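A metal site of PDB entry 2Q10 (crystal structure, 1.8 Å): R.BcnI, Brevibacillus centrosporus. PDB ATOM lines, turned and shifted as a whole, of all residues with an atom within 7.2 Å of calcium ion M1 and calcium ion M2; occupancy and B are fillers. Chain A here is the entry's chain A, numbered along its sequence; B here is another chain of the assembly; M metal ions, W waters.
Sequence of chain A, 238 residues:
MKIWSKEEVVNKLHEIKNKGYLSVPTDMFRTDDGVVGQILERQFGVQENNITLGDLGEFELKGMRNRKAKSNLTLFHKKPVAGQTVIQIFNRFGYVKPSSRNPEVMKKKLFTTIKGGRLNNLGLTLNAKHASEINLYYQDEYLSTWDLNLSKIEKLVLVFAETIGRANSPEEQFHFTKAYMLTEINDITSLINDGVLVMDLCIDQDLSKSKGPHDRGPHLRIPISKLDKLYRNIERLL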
ATOM      1  N   GLY A  37      27.816  -4.976   2.569  1.00  0.00           N
ATOM      2  CA  GLY A  37      27.418  -5.093   1.169  1.00  0.00           C
ATOM      3  C   GLY A  37      27.643  -3.787   0.441  1.00  0.00           C
ATOM      4  O   GLY A  37      28.072  -3.791  -0.704  1.00  0.00           O
ATOM      5  N   GLU A  41      30.233  -3.310  -2.686  1.00  0.00           N
ATOM      6  CA  GLU A  41      29.773  -2.689  -3.946  1.00  0.00           C
ATOM      7  C   GLU A  41      30.675  -1.564  -4.409  1.00  0.00           C
ATOM      8  O   GLU A  41      31.017  -1.443  -5.602  1.00  0.00           O
ATOM      9  CB  GLU A  41      28.342  -2.167  -3.794  1.00  0.00           C
ATOM     10  CG  GLU A  41      27.306  -3.261  -3.800  1.00  0.00           C
ATOM     11  CD  GLU A  41      25.911  -2.758  -3.679  1.00  0.00           C
ATOM     12  OE1 GLU A  41      25.689  -1.690  -3.065  1.00  0.00           O
ATOM     13  OE2 GLU A  41      25.006  -3.439  -4.191  1.00  0.00           O
ATOM     14  N   VAL A  46      29.900  -0.516  -8.224  1.00  0.00           N
ATOM     15  CA  VAL A  46      28.483  -0.779  -8.439  1.00  0.00           C
ATOM     16  C   VAL A  46      27.688   0.423  -7.886  1.00  0.00           C
ATOM     17  O   VAL A  46      27.620   0.616  -6.669  1.00  0.00           O
ATOM     18  CB  VAL A  46      28.063  -2.097  -7.731  1.00  0.00           C
ATOM     19  CG1 VAL A  46      26.547  -2.277  -7.716  1.00  0.00           C
ATOM     20  CG2 VAL A  46      28.737  -3.298  -8.400  1.00  0.00           C
ATOM     21  N   GLU A  48      24.450   1.586  -8.768  1.00  0.00           N
ATOM     22  CA  GLU A  48      23.041   1.400  -8.491  1.00  0.00           C
ATOM     23  C   GLU A  48      22.659  -0.028  -8.789  1.00  0.00           C
ATOM     24  O   GLU A  48      23.391  -0.745  -9.510  1.00  0.00           O
ATOM     25  CB  GLU A  48      22.193   2.384  -9.324  1.00  0.00           C
ATOM     26  CG  GLU A  48      22.345   2.254 -10.846  1.00  0.00           C
ATOM     27  CD  GLU A  48      21.612   3.352 -11.580  1.00  0.00           C
ATOM     28  OE1 GLU A  48      22.067   3.726 -12.673  1.00  0.00           O
ATOM     29  OE2 GLU A  48      20.590   3.841 -11.060  1.00  0.00           O
ATOM     30  N   ASN A  49      21.508  -0.440  -8.245  1.00  0.00           N
ATOM     31  CA  ASN A  49      20.887  -1.693  -8.636  1.00  0.00           C
ATOM     32  C   ASN A  49      20.495  -1.657 -10.113  1.00  0.00           C
ATOM     33  O   ASN A  49      20.058  -0.624 -10.626  1.00  0.00           O
ATOM     34  CB  ASN A  49      19.631  -1.985  -7.806  1.00  0.00           C
ATOM     35  CG  ASN A  49      19.047  -3.344  -8.113  1.00  0.00           C
ATOM     36  OD1 ASN A  49      19.730  -4.360  -7.969  1.00  0.00           O
ATOM     37  ND2 ASN A  49      17.793  -3.377  -8.566  1.00  0.00           N
ATOM     38  N   ASN A  50      20.652  -2.788 -10.780  1.00  0.00           N
ATOM     39  CA  ASN A  50      20.152  -2.959 -12.146  1.00  0.00           C
ATOM     40  C   ASN A  50      19.022  -3.975 -12.133  1.00  0.00           C
ATOM     41  O   ASN A  50      19.161  -5.054 -11.575  1.00  0.00           O
ATOM     42  CB  ASN A  50      21.294  -3.427 -13.068  1.00  0.00           C
ATOM     43  CG  ASN A  50      20.890  -3.421 -14.527  1.00  0.00           C
ATOM     44  OD1 ASN A  50      20.150  -4.295 -14.986  1.00  0.00           O
ATOM     45  ND2 ASN A  50      21.367  -2.425 -15.271  1.00  0.00           N
ATOM     46  N   LEU A  53      19.884  -7.548 -14.409  1.00  0.00           N
ATOM     47  CA  LEU A  53      21.074  -8.389 -14.258  1.00  0.00           C
ATOM     48  C   LEU A  53      21.647  -8.360 -12.845  1.00  0.00           C
ATOM     49  O   LEU A  53      21.533  -7.356 -12.145  1.00  0.00           O
ATOM     50  CB  LEU A  53      22.158  -7.860 -15.203  1.00  0.00           C
ATOM     51  CG  LEU A  53      21.804  -7.741 -16.693  1.00  0.00           C
ATOM     52  CD1 LEU A  53      23.022  -7.182 -17.412  1.00  0.00           C
ATOM     53  CD2 LEU A  53      21.370  -9.098 -17.247  1.00  0.00           C
ATOM     54  N   GLY A  54      22.309  -9.460 -12.461  1.00  0.00           N
ATOM     55  CA  GLY A  54      23.228  -9.455 -11.310  1.00  0.00           C
ATOM     56  C   GLY A  54      24.183  -8.256 -11.365  1.00  0.00           C
ATOM     57  O   GLY A  54      24.516  -7.777 -12.443  1.00  0.00           O
ATOM     58  N   ASP A  55      24.643  -7.815 -10.196  1.00  0.00           N
ATOM     59  CA  ASP A  55      25.374  -6.553 -10.056  1.00  0.00           C
ATOM     60  C   ASP A  55      26.578  -6.436 -10.944  1.00  0.00           C
ATOM     61  O   ASP A  55      26.971  -5.322 -11.287  1.00  0.00           O
ATOM     62  CB  ASP A  55      25.950  -6.360  -8.663  1.00  0.00           C
ATOM     63  CG  ASP A  55      24.914  -6.331  -7.604  1.00  0.00           C
ATOM     64  OD1 ASP A  55      24.089  -5.398  -7.587  1.00  0.00           O
ATOM     65  OD2 ASP A  55      24.955  -7.224  -6.761  1.00  0.00           O
ATOM     66  N   LEU A  56      27.220  -7.562 -11.248  1.00  0.00           N
ATOM     67  CA  LEU A  56      28.463  -7.559 -12.009  1.00  0.00           C
ATOM     68  C   LEU A  56      28.258  -7.891 -13.494  1.00  0.00           C
ATOM     69  O   LEU A  56      29.221  -7.874 -14.264  1.00  0.00           O
ATOM     70  CB  LEU A  56      29.500  -8.516 -11.370  1.00  0.00           C
ATOM     71  CG  LEU A  56      29.885  -8.264  -9.899  1.00  0.00           C
ATOM     72  CD1 LEU A  56      30.884  -9.296  -9.365  1.00  0.00           C
ATOM     73  CD2 LEU A  56      30.486  -6.854  -9.730  1.00  0.00           C
ATOM     74  N   PHE A  59      27.355 -12.103 -13.133  1.00  0.00           N
ATOM     75  CA  PHE A  59      27.329 -12.562 -11.738  1.00  0.00           C
ATOM     76  C   PHE A  59      26.631 -11.549 -10.847  1.00  0.00           C
ATOM     77  O   PHE A  59      26.725 -10.332 -11.061  1.00  0.00           O
ATOM     78  CB  PHE A  59      28.742 -12.751 -11.197  1.00  0.00           C
ATOM     79  CG  PHE A  59      29.704 -13.324 -12.189  1.00  0.00           C
ATOM     80  CD1 PHE A  59      29.596 -14.644 -12.613  1.00  0.00           C
ATOM     81  CD2 PHE A  59      30.712 -12.540 -12.725  1.00  0.00           C
ATOM     82  CE1 PHE A  59      30.470 -15.150 -13.551  1.00  0.00           C
ATOM     83  CE2 PHE A  59      31.587 -13.029 -13.658  1.00  0.00           C
ATOM     84  CZ  PHE A  59      31.482 -14.340 -14.071  1.00  0.00           C
ATOM     85  N   GLU A  60      25.951 -12.084  -9.842  1.00  0.00           N
ATOM     86  CA  GLU A  60      25.350 -11.304  -8.772  1.00  0.00           C
ATOM     87  C   GLU A  60      26.358 -11.292  -7.604  1.00  0.00           C
ATOM     88  O   GLU A  60      26.858 -12.346  -7.193  1.00  0.00           O
ATOM     89  CB  GLU A  60      23.995 -11.923  -8.394  1.00  0.00           C
ATOM     90  CG  GLU A  60      23.366 -11.504  -7.055  1.00  0.00           C
ATOM     91  CD  GLU A  60      23.144 -10.018  -6.906  1.00  0.00           C
ATOM     92  OE1 GLU A  60      23.045  -9.293  -7.941  1.00  0.00           O
ATOM     93  OE2 GLU A  60      23.048  -9.577  -5.740  1.00  0.00           O
ATOM     94  N   LEU A  61      26.635 -10.102  -7.077  1.00  0.00           N
ATOM     95  CA  LEU A  61      27.625  -9.920  -6.022  1.00  0.00           C
ATOM     96  C   LEU A  61      26.956  -9.942  -4.652  1.00  0.00           C
ATOM     97  O   LEU A  61      25.955  -9.245  -4.453  1.00  0.00           O
ATOM     98  CB  LEU A  61      28.329  -8.576  -6.190  1.00  0.00           C
ATOM     99  CG  LEU A  61      29.396  -8.145  -5.170  1.00  0.00           C
ATOM    100  CD1 LEU A  61      30.686  -8.998  -5.240  1.00  0.00           C
ATOM    101  CD2 LEU A  61      29.705  -6.658  -5.390  1.00  0.00           C
ATOM    102  N   LYS A  62      27.544 -10.708  -3.728  1.00  0.00           N
ATOM    103  CA  LYS A  62      27.075 -10.791  -2.355  1.00  0.00           C
ATOM    104  C   LYS A  62      28.227 -10.769  -1.365  1.00  0.00           C
ATOM    105  O   LYS A  62      29.219 -11.471  -1.529  1.00  0.00           O
ATOM    106  CB  LYS A  62      26.208 -12.040  -2.144  1.00  0.00           C
ATOM    107  CG  LYS A  62      24.988 -12.038  -3.061  1.00  0.00           C
ATOM    108  CD  LYS A  62      23.686 -12.303  -2.425  1.00  0.00           C
ATOM    109  CE  LYS A  62      22.576 -12.365  -3.496  1.00  0.00           C
ATOM    110  NZ  LYS A  62      21.636 -11.189  -3.560  1.00  0.00           N
ATOM    111  N   GLY A  63      28.084  -9.944  -0.337  1.00  0.00           N
ATOM    112  CA  GLY A  63      29.053  -9.863   0.749  1.00  0.00           C
ATOM    113  C   GLY A  63      28.421 -10.395   2.027  1.00  0.00           C
ATOM    114  O   GLY A  63      27.202 -10.302   2.214  1.00  0.00           O
ATOM    115  N   LEU A  75      19.031 -13.954  -1.052  1.00  0.00           N
ATOM    116  CA  LEU A  75      19.239 -14.110  -2.514  1.00  0.00           C
ATOM    117  C   LEU A  75      18.587 -12.932  -3.269  1.00  0.00           C
ATOM    118  O   LEU A  75      19.227 -12.261  -4.094  1.00  0.00           O
ATOM    119  CB  LEU A  75      18.690 -15.469  -2.951  1.00  0.00           C
ATOM    120  CG  LEU A  75      19.426 -16.666  -2.324  1.00  0.00           C
ATOM    121  CD1 LEU A  75      18.649 -17.983  -2.482  1.00  0.00           C
ATOM    122  CD2 LEU A  75      20.839 -16.797  -2.877  1.00  0.00           C
ATOM    123  N   LYS A 152      18.626 -13.571 -11.896  1.00  0.00           N
ATOM    124  CA  LYS A 152      19.767 -12.795 -11.415  1.00  0.00           C
ATOM    125  C   LYS A 152      20.746 -13.594 -10.553  1.00  0.00           C
ATOM    126  O   LYS A 152      21.894 -13.201 -10.443  1.00  0.00           O
ATOM    127  CB  LYS A 152      19.336 -11.547 -10.647  1.00  0.00           C
ATOM    128  CG  LYS A 152      18.950 -10.364 -11.562  1.00  0.00           C
ATOM    129  CD  LYS A 152      18.444  -9.150 -10.764  1.00  0.00           C
ATOM    130  CE  LYS A 152      19.540  -8.477  -9.909  1.00  0.00           C
ATOM    131  NZ  LYS A 152      19.312  -6.987  -9.715  1.00  0.00           N
ATOM    132  N   VAL A 157      28.891 -14.376  -7.035  1.00  0.00           N
ATOM    133  CA  VAL A 157      30.210 -14.128  -6.457  1.00  0.00           C
ATOM    134  C   VAL A 157      29.925 -13.707  -5.011  1.00  0.00           C
ATOM    135  O   VAL A 157      29.391 -12.625  -4.757  1.00  0.00           O
ATOM    136  CB  VAL A 157      31.019 -13.045  -7.242  1.00  0.00           C
ATOM    137  CG1 VAL A 157      32.278 -12.648  -6.452  1.00  0.00           C
ATOM    138  CG2 VAL A 157      31.389 -13.534  -8.667  1.00  0.00           C
ATOM    139  P    DC B   4      15.884  -7.172  -5.481  1.00  0.00           P
ATOM    140  OP1  DC B   4      16.657  -7.715  -6.621  1.00  0.00           O
ATOM    141  OP2  DC B   4      15.416  -8.083  -4.400  1.00  0.00           O
ATOM    142  O5'  DC B   4      16.741  -6.007  -4.797  1.00  0.00           O
ATOM    143  C5'  DC B   4      17.374  -5.012  -5.592  1.00  0.00           C
ATOM    144  C4'  DC B   4      18.124  -4.045  -4.711  1.00  0.00           C
ATOM    145  O4'  DC B   4      17.204  -3.344  -3.851  1.00  0.00           O
ATOM    146  C3'  DC B   4      19.077  -4.711  -3.735  1.00  0.00           C
ATOM    147  O3'  DC B   4      20.313  -5.038  -4.379  1.00  0.00           O
ATOM    148  C2'  DC B   4      19.273  -3.629  -2.691  1.00  0.00           C
ATOM    149  C1'  DC B   4      17.874  -3.012  -2.624  1.00  0.00           C
ATOM    150  N1   DC B   4      17.045  -3.492  -1.511  1.00  0.00           N
ATOM    151  C2   DC B   4      17.357  -3.040  -0.226  1.00  0.00           C
ATOM    152  O2   DC B   4      18.360  -2.328  -0.072  1.00  0.00           O
ATOM    153  N3   DC B   4      16.571  -3.412   0.817  1.00  0.00           N
ATOM    154  C4   DC B   4      15.514  -4.205   0.613  1.00  0.00           C
ATOM    155  N4   DC B   4      14.751  -4.500   1.661  1.00  0.00           N
ATOM    156  C5   DC B   4      15.201  -4.706  -0.688  1.00  0.00           C
ATOM    157  C6   DC B   4      15.988  -4.330  -1.707  1.00  0.00           C
ATOM    158  P    DC B   5      21.221  -6.226  -3.798  1.00  0.00           P
ATOM    159  OP1  DC B   5      22.422  -6.290  -4.670  1.00  0.00           O
ATOM    160  OP2  DC B   5      20.373  -7.427  -3.621  1.00  0.00           O
ATOM    161  O5'  DC B   5      21.648  -5.706  -2.368  1.00  0.00           O
ATOM    162  C5'  DC B   5      22.607  -4.658  -2.239  1.00  0.00           C
ATOM    163  C4'  DC B   5      22.911  -4.408  -0.780  1.00  0.00           C
ATOM    164  O4'  DC B   5      21.792  -3.803  -0.095  1.00  0.00           O
ATOM    165  C3'  DC B   5      23.211  -5.643   0.052  1.00  0.00           C
ATOM    166  O3'  DC B   5      24.521  -6.153  -0.234  1.00  0.00           O
ATOM    167  C2'  DC B   5      23.093  -5.064   1.447  1.00  0.00           C
ATOM    168  C1'  DC B   5      21.849  -4.173   1.289  1.00  0.00           C
ATOM    169  N1   DC B   5      20.600  -4.857   1.625  1.00  0.00           N
ATOM    170  C2   DC B   5      20.173  -4.849   2.959  1.00  0.00           C
ATOM    171  O2   DC B   5      20.861  -4.261   3.791  1.00  0.00           O
ATOM    172  N3   DC B   5      19.029  -5.503   3.298  1.00  0.00           N
ATOM    173  C4   DC B   5      18.318  -6.127   2.354  1.00  0.00           C
ATOM    174  N4   DC B   5      17.199  -6.745   2.731  1.00  0.00           N
ATOM    175  C5   DC B   5      18.721  -6.139   0.992  1.00  0.00           C
ATOM    176  C6   DC B   5      19.858  -5.502   0.668  1.00  0.00           C
ATOM    177  P    DG B   6      24.938  -7.612   0.265  1.00  0.00           P
ATOM    178  OP1  DG B   6      26.313  -7.855  -0.225  1.00  0.00           O
ATOM    179  OP2  DG B   6      23.852  -8.558  -0.105  1.00  0.00           O
ATOM    180  O5'  DG B   6      24.941  -7.446   1.846  1.00  0.00           O
ATOM    181  C5'  DG B   6      24.571  -8.506   2.714  1.00  0.00           C
ATOM    182  C4'  DG B   6      24.082  -7.917   4.017  1.00  0.00           C
ATOM    183  O4'  DG B   6      22.712  -7.499   3.911  1.00  0.00           O
ATOM    184  C3'  DG B   6      24.087  -8.859   5.215  1.00  0.00           C
ATOM    185  O3'  DG B   6      25.427  -8.971   5.686  1.00  0.00           O
ATOM    186  C2'  DG B   6      23.188  -8.093   6.174  1.00  0.00           C
ATOM    187  C1'  DG B   6      22.131  -7.506   5.217  1.00  0.00           C
ATOM    188  N9   DG B   6      20.925  -8.322   5.155  1.00  0.00           N
ATOM    189  C8   DG B   6      20.480  -9.086   4.101  1.00  0.00           C
ATOM    190  N7   DG B   6      19.392  -9.757   4.383  1.00  0.00           N
ATOM    191  C5   DG B   6      19.100  -9.399   5.687  1.00  0.00           C
ATOM    192  C6   DG B   6      18.058  -9.808   6.542  1.00  0.00           C
ATOM    193  O6   DG B   6      17.155 -10.618   6.319  1.00  0.00           O
ATOM    194  N1   DG B   6      18.133  -9.189   7.778  1.00  0.00           N
ATOM    195  C2   DG B   6      19.096  -8.288   8.152  1.00  0.00           C
ATOM    196  N2   DG B   6      19.000  -7.793   9.396  1.00  0.00           N
ATOM    197  N3   DG B   6      20.085  -7.898   7.373  1.00  0.00           N
ATOM    198  C4   DG B   6      20.032  -8.489   6.165  1.00  0.00           C
HETATM  199 CA    CA M   1      24.202  -7.765  -4.859  1.00  0.00          CA
HETATM  200 CA    CA M   2      21.959  -5.148  -6.978  1.00  0.00          CA
HETATM  201  O   HOH W   1      22.603  -3.149  -6.116  1.00  0.00           O
HETATM  202  O   HOH W   2      23.177  -8.604  -2.848  1.00  0.00           O
HETATM  203  O   HOH W   3      25.491  -6.150  -4.006  1.00  0.00           O
HETATM  204  O   HOH W   4      21.455  -7.181  -7.620  1.00  0.00           O
HETATM  205  O   HOH W   5      23.770  -3.420  -9.232  1.00  0.00           O
HETATM  206  O   HOH W   6      22.133  -5.458 -10.299  1.00  0.00           O
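Water W2 lies within hydrogen-bond range of OP2 of DG 6 of chain B (2.8 Å), NZ of Lys 62 (3.1 Å) and OP2 of DC 5 of chain B (3.1 Å).
Water W1 lies within hydrogen-bond range of OE2 of Glu 41 (3.1 Å) and O3' of DC 4 of chain B (3.4 Å).
Water W4 bridges OE1 of Glu 60 (2.7 Å) and NZ of Lys 152 (3.0 Å).
Calcium ion M1 is bound by the side-chain carboxylate (OD2) of Asp 55 (2.1 Å), water W3 (2.2 Å), OP1 of DC 5 of chain B (2.3 Å), the side-chain carboxylate (OE2) of Glu 60 (2.3 Å), the backbone carbonyl oxygen (O) of Leu 61 (2.3 Å) and water W2 (2.4 Å).
Calcium ion M1 has six donor atoms within binding distance.
OP2 of DC 5 of chain B is in salt-bridge range of the side-chain amino group of Lys 62.
The side-chain carboxylate of Glu 60 lies close to the side-chain amino group of Lys 62, at 3.1 Å.
O of Glu 60 is in hydrogen-bond range of N of Val 157, at 2.9 Å.
The side-chain amino group (NZ) of Lys 152 sits close to the side-chain amide oxygen (OD1) of Asn 49.
Four residues have an atom within 4 Å of calcium ion M2: Asn 49, Asp 55, DC 4 of chain B and DC 5 of chain B.
Calcium ion M2 is bound by water W4, OD1 of Asp 55, water W1, OD1 of Asn 49 and OP1 of DC 5 of chain B.
Calcium ion M2 has five donor atoms within binding distance.
Slightly farther from calcium ion M2 lies O3' of DC 4 of chain B (3.1 Å).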
